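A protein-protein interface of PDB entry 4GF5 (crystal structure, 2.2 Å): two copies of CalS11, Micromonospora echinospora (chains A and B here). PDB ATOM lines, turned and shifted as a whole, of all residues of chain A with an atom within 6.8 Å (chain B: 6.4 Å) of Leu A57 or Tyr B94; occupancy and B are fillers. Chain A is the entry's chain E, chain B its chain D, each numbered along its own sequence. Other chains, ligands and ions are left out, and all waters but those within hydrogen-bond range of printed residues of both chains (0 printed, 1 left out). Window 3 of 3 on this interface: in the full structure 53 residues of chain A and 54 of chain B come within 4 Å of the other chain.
OD2 of Asp B60 lies within salt-bridge range of NE of Arg B64, at 2.8 Å.
The backbone carbonyl oxygen (O) of Thr A54 is in hydrogen-bond range of the side-chain hydroxyl (OG) of Ser A58 (3.0 Å).
The side-chain carboxylate (OD2) of Asp A60 lies within salt-bridge range of the guanidinium group (NE) of Arg A64 (2.8 Å).
OD1 of Asp B60 sits at hydrogen-bond distance from OH of Tyr B94, 2.6 Å away.
O of Arg A50 lies within hydrogen-bond range of OG1 of Thr A54, 2.7 Å away.
Gly B92 touches Arg A50.
Arg A50 touches Val B93 (CG to N, 3.7 Å).
Met A53 touches Leu B56 (SD to CD2, 3.8 Å).
Met A53 touches Leu B90.
Thr A54 touches Val B93.
Leu A56 touches Leu B56 (CD1 to CD1, 3.8 Å).
CD2 of Leu A57 touches CG of Asp B60, at 3.7 Å.
CD1 of Leu A57 touches CD2 of Leu B90, 3.9 Å away.
CD1 of Leu A57 touches OH of Tyr B94, 3.9 Å away.
CD2 of Leu B57 touches CG of Asp A60, 3.8 Å away.
Of the printed residues of chain A, Gly B92 touches Arg A50 (3.5 Å).
Printed residues of chain A within 4 Å of Leu B90: Met A53 and Leu A57.
Pro B96 touches none of the printed residues of chain A.
Ala B89 touches none of the printed residues of chain A.
The nearest residue of chain B that does not touch Leu A57 is Val B93 (4.1 Å).
Hydrophobic or aromatic side chains of chain A within 4 Å of the printed part of chain B: Met A53, Leu A56 and Leu A57.
Of the 15 printed residues of chain B, 7 touch a printed residue of chain A.
Hydrophobic or aromatic side chains of chain B that line the printed part of chain A: Leu B56, Leu B57, Leu B90, Val B93 and Tyr B94.
Among the printed residues, 11 pairs touch across the chains.
Among the printed residues, no Asp or Glu carboxylate lies within 4 Å of a Lys or Arg side-chain nitrogen of the other chain.
Leu B56 touches its own counterpart, Leu A56.
Leu A57 touches Asp B60, and with the chains exchanged Asp A60 touches Leu B57.
4 positions are printed for both chains.
Of the 11 pairs that touch across the chains among the printed residues, 3 have their exchanged pair printed and touching as well.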
ATOM      1  N   ARG A  50      12.503   6.060  24.640  1.00  0.00           N
ATOM      2  CA  ARG A  50      11.796   4.774  24.516  1.00  0.00           C
ATOM      3  C   ARG A  50      10.281   4.902  24.441  1.00  0.00           C
ATOM      4  O   ARG A  50       9.661   4.393  23.507  1.00  0.00           O
ATOM      5  CB  ARG A  50      12.133   3.840  25.681  1.00  0.00           C
ATOM      6  CG  ARG A  50      11.318   2.524  25.682  1.00  0.00           C
ATOM      7  CD  ARG A  50      11.395   1.760  27.038  1.00  0.00           C
ATOM      8  NE  ARG A  50      10.876   2.561  28.141  1.00  0.00           N
ATOM      9  CZ  ARG A  50       9.580   2.782  28.364  1.00  0.00           C
ATOM     10  NH1 ARG A  50       8.656   2.242  27.575  1.00  0.00           N
ATOM     11  NH2 ARG A  50       9.197   3.532  29.383  1.00  0.00           N
ATOM     12  N   GLN A  52       8.342   7.372  23.678  1.00  0.00           N
ATOM     13  CA  GLN A  52       7.844   8.017  22.457  1.00  0.00           C
ATOM     14  C   GLN A  52       8.168   7.212  21.201  1.00  0.00           C
ATOM     15  O   GLN A  52       7.376   7.171  20.250  1.00  0.00           O
ATOM     16  CB  GLN A  52       8.380   9.450  22.314  1.00  0.00           C
ATOM     17  CG  GLN A  52       7.959  10.393  23.431  1.00  0.00           C
ATOM     18  CD  GLN A  52       6.444  10.454  23.616  1.00  0.00           C
ATOM     19  OE1 GLN A  52       5.675  10.277  22.669  1.00  0.00           O
ATOM     20  NE2 GLN A  52       6.014  10.699  24.843  1.00  0.00           N
ATOM     21  N   MET A  53       9.340   6.590  21.196  1.00  0.00           N
ATOM     22  CA  MET A  53       9.712   5.695  20.113  1.00  0.00           C
ATOM     23  C   MET A  53       8.683   4.569  20.021  1.00  0.00           C
ATOM     24  O   MET A  53       8.271   4.187  18.931  1.00  0.00           O
ATOM     25  CB  MET A  53      11.106   5.111  20.354  1.00  0.00           C
ATOM     26  CG  MET A  53      11.478   3.976  19.403  1.00  0.00           C
ATOM     27  SD  MET A  53      11.767   4.559  17.715  1.00  0.00           S
ATOM     28  CE  MET A  53      13.487   5.039  17.791  1.00  0.00           C
ATOM     29  N   THR A  54       8.258   4.055  21.173  1.00  0.00           N
ATOM     30  CA  THR A  54       7.286   2.962  21.219  1.00  0.00           C
ATOM     31  C   THR A  54       5.985   3.374  20.534  1.00  0.00           C
ATOM     32  O   THR A  54       5.414   2.619  19.738  1.00  0.00           O
ATOM     33  CB  THR A  54       6.980   2.526  22.666  1.00  0.00           C
ATOM     34  OG1 THR A  54       8.190   2.107  23.304  1.00  0.00           O
ATOM     35  CG2 THR A  54       5.984   1.362  22.687  1.00  0.00           C
ATOM     36  N   ASP A  55       5.527   4.581  20.848  1.00  0.00           N
ATOM     37  CA  ASP A  55       4.325   5.133  20.235  1.00  0.00           C
ATOM     38  C   ASP A  55       4.457   5.161  18.722  1.00  0.00           C
ATOM     39  O   ASP A  55       3.537   4.795  18.003  1.00  0.00           O
ATOM     40  CB  ASP A  55       4.093   6.555  20.727  1.00  0.00           C
ATOM     41  CG  ASP A  55       2.934   7.221  20.039  1.00  0.00           C
ATOM     42  OD1 ASP A  55       1.789   6.881  20.408  1.00  0.00           O
ATOM     43  OD2 ASP A  55       3.165   8.082  19.141  1.00  0.00           O
ATOM     44  N   LEU A  56       5.614   5.602  18.256  1.00  0.00           N
ATOM     45  CA  LEU A  56       5.870   5.743  16.842  1.00  0.00           C
ATOM     46  C   LEU A  56       5.835   4.362  16.189  1.00  0.00           C
ATOM     47  O   LEU A  56       5.302   4.197  15.093  1.00  0.00           O
ATOM     48  CB  LEU A  56       7.231   6.412  16.631  1.00  0.00           C
ATOM     49  CG  LEU A  56       7.633   6.815  15.211  1.00  0.00           C
ATOM     50  CD1 LEU A  56       8.765   7.829  15.268  1.00  0.00           C
ATOM     51  CD2 LEU A  56       8.073   5.617  14.412  1.00  0.00           C
ATOM     52  N   LEU A  57       6.439   3.379  16.845  1.00  0.00           N
ATOM     53  CA  LEU A  57       6.509   2.039  16.284  1.00  0.00           C
ATOM     54  C   LEU A  57       5.104   1.438  16.211  1.00  0.00           C
ATOM     55  O   LEU A  57       4.765   0.744  15.258  1.00  0.00           O
ATOM     56  CB  LEU A  57       7.471   1.154  17.097  1.00  0.00           C
ATOM     57  CG  LEU A  57       8.967   1.503  16.941  1.00  0.00           C
ATOM     58  CD1 LEU A  57       9.840   0.733  17.905  1.00  0.00           C
ATOM     59  CD2 LEU A  57       9.472   1.276  15.508  1.00  0.00           C
ATOM     60  N   SER A  58       4.276   1.742  17.202  1.00  0.00           N
ATOM     61  CA  SER A  58       2.905   1.263  17.200  1.00  0.00           C
ATOM     62  C   SER A  58       2.092   1.855  16.042  1.00  0.00           C
ATOM     63  O   SER A  58       1.369   1.124  15.359  1.00  0.00           O
ATOM     64  CB  SER A  58       2.221   1.533  18.541  1.00  0.00           C
ATOM     65  OG  SER A  58       2.915   0.890  19.599  1.00  0.00           O
ATOM     66  N   MET A  59       2.200   3.162  15.820  1.00  0.00           N
ATOM     67  CA  MET A  59       1.497   3.782  14.704  1.00  0.00           C
ATOM     68  C   MET A  59       1.924   3.147  13.383  1.00  0.00           C
ATOM     69  O   MET A  59       1.089   2.850  12.528  1.00  0.00           O
ATOM     70  CB  MET A  59       1.718   5.295  14.669  1.00  0.00           C
ATOM     71  CG  MET A  59       1.179   6.059  15.881  1.00  0.00           C
ATOM     72  SD  MET A  59      -0.566   5.761  16.292  1.00  0.00           S
ATOM     73  CE  MET A  59      -0.374   4.718  17.744  1.00  0.00           C
ATOM     74  N   ASP A  60       3.227   2.921  13.232  1.00  0.00           N
ATOM     75  CA  ASP A  60       3.752   2.262  12.038  1.00  0.00           C
ATOM     76  C   ASP A  60       3.150   0.883  11.861  1.00  0.00           C
ATOM     77  O   ASP A  60       2.753   0.523  10.758  1.00  0.00           O
ATOM     78  CB  ASP A  60       5.275   2.149  12.078  1.00  0.00           C
ATOM     79  CG  ASP A  60       5.830   1.368  10.887  1.00  0.00           C
ATOM     80  OD1 ASP A  60       5.714   1.866   9.746  1.00  0.00           O
ATOM     81  OD2 ASP A  60       6.378   0.258  11.078  1.00  0.00           O
ATOM     82  N   ALA A  61       3.101   0.116  12.954  1.00  0.00           N
ATOM     83  CA  ALA A  61       2.490  -1.210  12.949  1.00  0.00           C
ATOM     84  C   ALA A  61       1.027  -1.133  12.514  1.00  0.00           C
ATOM     85  O   ALA A  61       0.571  -1.963  11.737  1.00  0.00           O
ATOM     86  CB  ALA A  61       2.611  -1.861  14.324  1.00  0.00           C
ATOM     87  N   LEU A  62       0.287  -0.133  12.994  1.00  0.00           N
ATOM     88  CA  LEU A  62      -1.117  -0.019  12.600  1.00  0.00           C
ATOM     89  C   LEU A  62      -1.240   0.342  11.119  1.00  0.00           C
ATOM     90  O   LEU A  62      -2.002  -0.282  10.384  1.00  0.00           O
ATOM     91  CB  LEU A  62      -1.854   0.996  13.468  1.00  0.00           C
ATOM     92  CG  LEU A  62      -1.888   0.692  14.970  1.00  0.00           C
ATOM     93  CD1 LEU A  62      -2.643   1.775  15.714  1.00  0.00           C
ATOM     94  CD2 LEU A  62      -2.489  -0.673  15.265  1.00  0.00           C
ATOM     95  N   ARG A  64       0.789  -0.227   8.741  1.00  0.00           N
ATOM     96  CA  ARG A  64       1.173  -1.344   7.899  1.00  0.00           C
ATOM     97  C   ARG A  64       0.034  -2.352   7.727  1.00  0.00           C
ATOM     98  O   ARG A  64      -0.021  -3.065   6.740  1.00  0.00           O
ATOM     99  CB  ARG A  64       2.447  -2.023   8.424  1.00  0.00           C
ATOM    100  CG  ARG A  64       3.699  -1.222   8.127  1.00  0.00           C
ATOM    101  CD  ARG A  64       4.987  -1.936   8.495  1.00  0.00           C
ATOM    102  NE  ARG A  64       5.222  -1.981   9.935  1.00  0.00           N
ATOM    103  CZ  ARG A  64       5.167  -3.096  10.657  1.00  0.00           C
ATOM    104  NH1 ARG A  64       4.875  -4.254  10.064  1.00  0.00           N
ATOM    105  NH2 ARG A  64       5.399  -3.055  11.968  1.00  0.00           N
ATOM    106  N   THR A  86       3.210  11.739  12.435  1.00  0.00           N
ATOM    107  CA  THR A  86       3.669  10.376  12.192  1.00  0.00           C
ATOM    108  C   THR A  86       2.991   9.807  10.940  1.00  0.00           C
ATOM    109  O   THR A  86       3.657   9.350  10.016  1.00  0.00           O
ATOM    110  CB  THR A  86       3.374   9.451  13.401  1.00  0.00           C
ATOM    111  OG1 THR A  86       3.938  10.009  14.591  1.00  0.00           O
ATOM    112  CG2 THR A  86       3.958   8.068  13.184  1.00  0.00           C
ATOM    113  N   LEU A 244      -0.294  -4.842  20.691  1.00  0.00           N
ATOM    114  CA  LEU A 244       1.009  -5.187  20.153  1.00  0.00           C
ATOM    115  C   LEU A 244       1.817  -5.603  21.375  1.00  0.00           C
ATOM    116  O   LEU A 244       1.937  -4.825  22.319  1.00  0.00           O
ATOM    117  CB  LEU A 244       1.636  -3.972  19.494  1.00  0.00           C
ATOM    118  CG  LEU A 244       0.729  -3.338  18.455  1.00  0.00           C
ATOM    119  CD1 LEU A 244       1.314  -2.013  18.037  1.00  0.00           C
ATOM    120  CD2 LEU A 244       0.624  -4.284  17.265  1.00  0.00           C
ATOM    121  N   ARG A 247       3.231  -3.756  24.965  1.00  0.00           N
ATOM    122  CA  ARG A 247       2.737  -2.389  25.071  1.00  0.00           C
ATOM    123  C   ARG A 247       1.303  -2.368  25.588  1.00  0.00           C
ATOM    124  O   ARG A 247       0.440  -3.050  25.048  1.00  0.00           O
ATOM    125  CB  ARG A 247       2.828  -1.702  23.704  1.00  0.00           C
ATOM    126  CG  ARG A 247       4.149  -2.000  23.024  1.00  0.00           C
ATOM    127  CD  ARG A 247       4.209  -1.557  21.588  1.00  0.00           C
ATOM    128  NE  ARG A 247       5.455  -2.029  20.987  1.00  0.00           N
ATOM    129  CZ  ARG A 247       5.844  -1.738  19.752  1.00  0.00           C
ATOM    130  NH1 ARG A 247       5.085  -0.962  18.994  1.00  0.00           N
ATOM    131  NH2 ARG A 247       6.994  -2.212  19.280  1.00  0.00           N
ATOM    132  N   LEU B  56      14.886   5.815  10.495  1.00  0.00           N
ATOM    133  CA  LEU B  56      14.479   5.265  11.777  1.00  0.00           C
ATOM    134  C   LEU B  56      13.871   3.862  11.593  1.00  0.00           C
ATOM    135  O   LEU B  56      14.222   2.940  12.315  1.00  0.00           O
ATOM    136  CB  LEU B  56      13.516   6.221  12.511  1.00  0.00           C
ATOM    137  CG  LEU B  56      13.011   5.899  13.931  1.00  0.00           C
ATOM    138  CD1 LEU B  56      12.415   7.130  14.598  1.00  0.00           C
ATOM    139  CD2 LEU B  56      11.977   4.776  13.967  1.00  0.00           C
ATOM    140  N   LEU B  57      12.963   3.702  10.632  1.00  0.00           N
ATOM    141  CA  LEU B  57      12.349   2.398  10.382  1.00  0.00           C
ATOM    142  C   LEU B  57      13.383   1.356   9.945  1.00  0.00           C
ATOM    143  O   LEU B  57      13.317   0.177  10.338  1.00  0.00           O
ATOM    144  CB  LEU B  57      11.204   2.524   9.369  1.00  0.00           C
ATOM    145  CG  LEU B  57      10.055   3.416   9.865  1.00  0.00           C
ATOM    146  CD1 LEU B  57       9.020   3.697   8.761  1.00  0.00           C
ATOM    147  CD2 LEU B  57       9.395   2.808  11.084  1.00  0.00           C
ATOM    148  N   ASP B  60      15.289   0.220  13.035  1.00  0.00           N
ATOM    149  CA  ASP B  60      14.416  -0.699  13.759  1.00  0.00           C
ATOM    150  C   ASP B  60      14.374  -2.072  13.093  1.00  0.00           C
ATOM    151  O   ASP B  60      14.415  -3.095  13.771  1.00  0.00           O
ATOM    152  CB  ASP B  60      13.003  -0.137  13.899  1.00  0.00           C
ATOM    153  CG  ASP B  60      12.050  -1.126  14.554  1.00  0.00           C
ATOM    154  OD1 ASP B  60      12.171  -1.309  15.780  1.00  0.00           O
ATOM    155  OD2 ASP B  60      11.175  -1.708  13.858  1.00  0.00           O
ATOM    156  N   TYR B  63      17.652  -3.894  13.840  1.00  0.00           N
ATOM    157  CA  TYR B  63      17.736  -4.254  15.259  1.00  0.00           C
ATOM    158  C   TYR B  63      16.897  -5.508  15.503  1.00  0.00           C
ATOM    159  O   TYR B  63      17.377  -6.486  16.115  1.00  0.00           O
ATOM    160  CB  TYR B  63      17.262  -3.091  16.140  1.00  0.00           C
ATOM    161  CG  TYR B  63      17.682  -3.156  17.602  1.00  0.00           C
ATOM    162  CD1 TYR B  63      17.511  -4.312  18.357  1.00  0.00           C
ATOM    163  CD2 TYR B  63      18.237  -2.055  18.230  1.00  0.00           C
ATOM    164  CE1 TYR B  63      17.890  -4.371  19.697  1.00  0.00           C
ATOM    165  CE2 TYR B  63      18.618  -2.106  19.569  1.00  0.00           C
ATOM    166  CZ  TYR B  63      18.448  -3.271  20.293  1.00  0.00           C
ATOM    167  OH  TYR B  63      18.829  -3.337  21.612  1.00  0.00           O
ATOM    168  N   ARG B  64      15.668  -5.495  14.981  1.00  0.00           N
ATOM    169  CA  ARG B  64      14.773  -6.631  15.113  1.00  0.00           C
ATOM    170  C   ARG B  64      15.392  -7.917  14.583  1.00  0.00           C
ATOM    171  O   ARG B  64      15.034  -8.996  15.029  1.00  0.00           O
ATOM    172  CB  ARG B  64      13.422  -6.366  14.442  1.00  0.00           C
ATOM    173  CG  ARG B  64      12.517  -5.421  15.234  1.00  0.00           C
ATOM    174  CD  ARG B  64      11.109  -5.325  14.625  1.00  0.00           C
ATOM    175  NE  ARG B  64      11.062  -4.514  13.408  1.00  0.00           N
ATOM    176  CZ  ARG B  64      10.790  -4.987  12.198  1.00  0.00           C
ATOM    177  NH1 ARG B  64      10.548  -6.286  12.033  1.00  0.00           N
ATOM    178  NH2 ARG B  64      10.757  -4.162  11.149  1.00  0.00           N
ATOM    179  N   LEU B  67      17.747  -9.529  17.524  1.00  0.00           N
ATOM    180  CA  LEU B  67      17.184  -9.674  18.853  1.00  0.00           C
ATOM    181  C   LEU B  67      17.482 -11.053  19.449  1.00  0.00           C
ATOM    182  O   LEU B  67      17.487 -11.197  20.669  1.00  0.00           O
ATOM    183  CB  LEU B  67      15.676  -9.423  18.841  1.00  0.00           C
ATOM    184  CG  LEU B  67      15.290  -7.955  18.678  1.00  0.00           C
ATOM    185  CD1 LEU B  67      13.793  -7.772  18.748  1.00  0.00           C
ATOM    186  CD2 LEU B  67      15.968  -7.134  19.772  1.00  0.00           C
ATOM    187  N   ALA B  89      17.150   4.193  22.204  1.00  0.00           N
ATOM    188  CA  ALA B  89      15.709   4.118  22.369  1.00  0.00           C
ATOM    189  C   ALA B  89      15.192   2.718  22.036  1.00  0.00           C
ATOM    190  O   ALA B  89      14.347   2.177  22.752  1.00  0.00           O
ATOM    191  CB  ALA B  89      15.007   5.176  21.522  1.00  0.00           C
ATOM    192  N   LEU B  90      15.701   2.123  20.958  1.00  0.00           N
ATOM    193  CA  LEU B  90      15.226   0.796  20.550  1.00  0.00           C
ATOM    194  C   LEU B  90      15.606  -0.264  21.564  1.00  0.00           C
ATOM    195  O   LEU B  90      14.820  -1.174  21.831  1.00  0.00           O
ATOM    196  CB  LEU B  90      15.738   0.403  19.161  1.00  0.00           C
ATOM    197  CG  LEU B  90      15.234   1.292  18.030  1.00  0.00           C
ATOM    198  CD1 LEU B  90      15.883   0.884  16.710  1.00  0.00           C
ATOM    199  CD2 LEU B  90      13.700   1.246  17.936  1.00  0.00           C
ATOM    200  N   ARG B  91      16.805  -0.143  22.123  1.00  0.00           N
ATOM    201  CA  ARG B  91      17.253  -1.061  23.161  1.00  0.00           C
ATOM    202  C   ARG B  91      16.291  -1.052  24.348  1.00  0.00           C
ATOM    203  O   ARG B  91      16.046  -2.087  24.961  1.00  0.00           O
ATOM    204  CB  ARG B  91      18.660  -0.713  23.626  1.00  0.00           C
ATOM    205  CG  ARG B  91      19.268  -1.781  24.524  1.00  0.00           C
ATOM    206  CD  ARG B  91      20.690  -1.431  24.894  1.00  0.00           C
ATOM    207  NE  ARG B  91      20.747  -0.115  25.512  1.00  0.00           N
ATOM    208  CZ  ARG B  91      21.863   0.576  25.699  1.00  0.00           C
ATOM    209  NH1 ARG B  91      23.031   0.077  25.310  1.00  0.00           N
ATOM    210  NH2 ARG B  91      21.803   1.773  26.271  1.00  0.00           N
ATOM    211  N   GLY B  92      15.740   0.118  24.660  1.00  0.00           N
ATOM    212  CA  GLY B  92      14.710   0.212  25.678  1.00  0.00           C
ATOM    213  C   GLY B  92      13.435  -0.518  25.269  1.00  0.00           C
ATOM    214  O   GLY B  92      12.868  -1.296  26.049  1.00  0.00           O
ATOM    215  N   VAL B  93      12.992  -0.274  24.040  1.00  0.00           N
ATOM    216  CA  VAL B  93      11.790  -0.911  23.508  1.00  0.00           C
ATOM    217  C   VAL B  93      11.899  -2.435  23.561  1.00  0.00           C
ATOM    218  O   VAL B  93      10.973  -3.117  23.988  1.00  0.00           O
ATOM    219  CB  VAL B  93      11.515  -0.482  22.037  1.00  0.00           C
ATOM    220  CG1 VAL B  93      10.359  -1.294  21.441  1.00  0.00           C
ATOM    221  CG2 VAL B  93      11.255   1.035  21.936  1.00  0.00           C
ATOM    222  N   TYR B  94      13.038  -2.970  23.140  1.00  0.00           N
ATOM    223  CA  TYR B  94      13.118  -4.399  22.915  1.00  0.00           C
ATOM    224  C   TYR B  94      13.817  -5.190  24.015  1.00  0.00           C
ATOM    225  O   TYR B  94      13.485  -6.350  24.255  1.00  0.00           O
ATOM    226  CB  TYR B  94      13.780  -4.692  21.567  1.00  0.00           C
ATOM    227  CG  TYR B  94      12.965  -4.248  20.380  1.00  0.00           C
ATOM    228  CD1 TYR B  94      11.759  -4.880  20.055  1.00  0.00           C
ATOM    229  CD2 TYR B  94      13.403  -3.207  19.568  1.00  0.00           C
ATOM    230  CE1 TYR B  94      11.006  -4.470  18.951  1.00  0.00           C
ATOM    231  CE2 TYR B  94      12.662  -2.787  18.478  1.00  0.00           C
ATOM    232  CZ  TYR B  94      11.466  -3.419  18.169  1.00  0.00           C
ATOM    233  OH  TYR B  94      10.748  -2.994  17.066  1.00  0.00           O
ATOM    234  N   GLU B  95      14.799  -4.582  24.668  1.00  0.00           N
ATOM    235  CA  GLU B  95      15.639  -5.342  25.583  1.00  0.00           C
ATOM    236  C   GLU B  95      15.873  -4.678  26.934  1.00  0.00           C
ATOM    237  O   GLU B  95      17.009  -4.410  27.295  1.00  0.00           O
ATOM    238  CB  GLU B  95      16.984  -5.613  24.932  1.00  0.00           C
ATOM    239  CG  GLU B  95      16.892  -6.310  23.590  1.00  0.00           C
ATOM    240  CD  GLU B  95      18.251  -6.667  23.050  1.00  0.00           C
ATOM    241  OE1 GLU B  95      18.989  -5.740  22.631  1.00  0.00           O
ATOM    242  OE2 GLU B  95      18.581  -7.872  23.049  1.00  0.00           O
ATOM    243  N   PRO B  96      14.806  -4.451  27.702  1.00  0.00           N
ATOM    244  CA  PRO B  96      14.980  -3.873  29.037  1.00  0.00           C
ATOM    245  C   PRO B  96      15.844  -4.754  29.944  1.00  0.00           C
ATOM    246  O   PRO B  96      16.470  -4.239  30.873  1.00  0.00           O
ATOM    247  CB  PRO B  96      13.551  -3.821  29.575  1.00  0.00           C
ATOM    248  CG  PRO B  96      12.831  -4.879  28.829  1.00  0.00           C
ATOM    249  CD  PRO B  96      13.413  -4.866  27.460  1.00  0.00           C
ATOM    250  N   TYR B  97      15.889  -6.058  29.670  1.00  0.00           N
ATOM    251  CA  TYR B  97      16.564  -6.982  30.560  1.00  0.00           C
ATOM    252  C   TYR B  97      17.926  -7.445  30.033  1.00  0.00           C
ATOM    253  O   TYR B  97      18.493  -8.412  30.552  1.00  0.00           O
ATOM    254  CB  TYR B  97      15.671  -8.191  30.862  1.00  0.00           C
ATOM    255  CG  TYR B  97      14.354  -7.842  31.529  1.00  0.00           C
ATOM    256  CD1 TYR B  97      14.319  -6.996  32.629  1.00  0.00           C
ATOM    257  CD2 TYR B  97      13.145  -8.350  31.055  1.00  0.00           C
ATOM    258  CE1 TYR B  97      13.137  -6.666  33.258  1.00  0.00           C
ATOM    259  CE2 TYR B  97      11.932  -8.024  31.687  1.00  0.00           C
ATOM    260  CZ  TYR B  97      11.943  -7.175  32.792  1.00  0.00           C
ATOM    261  OH  TYR B  97      10.776  -6.824  33.444  1.00  0.00           O
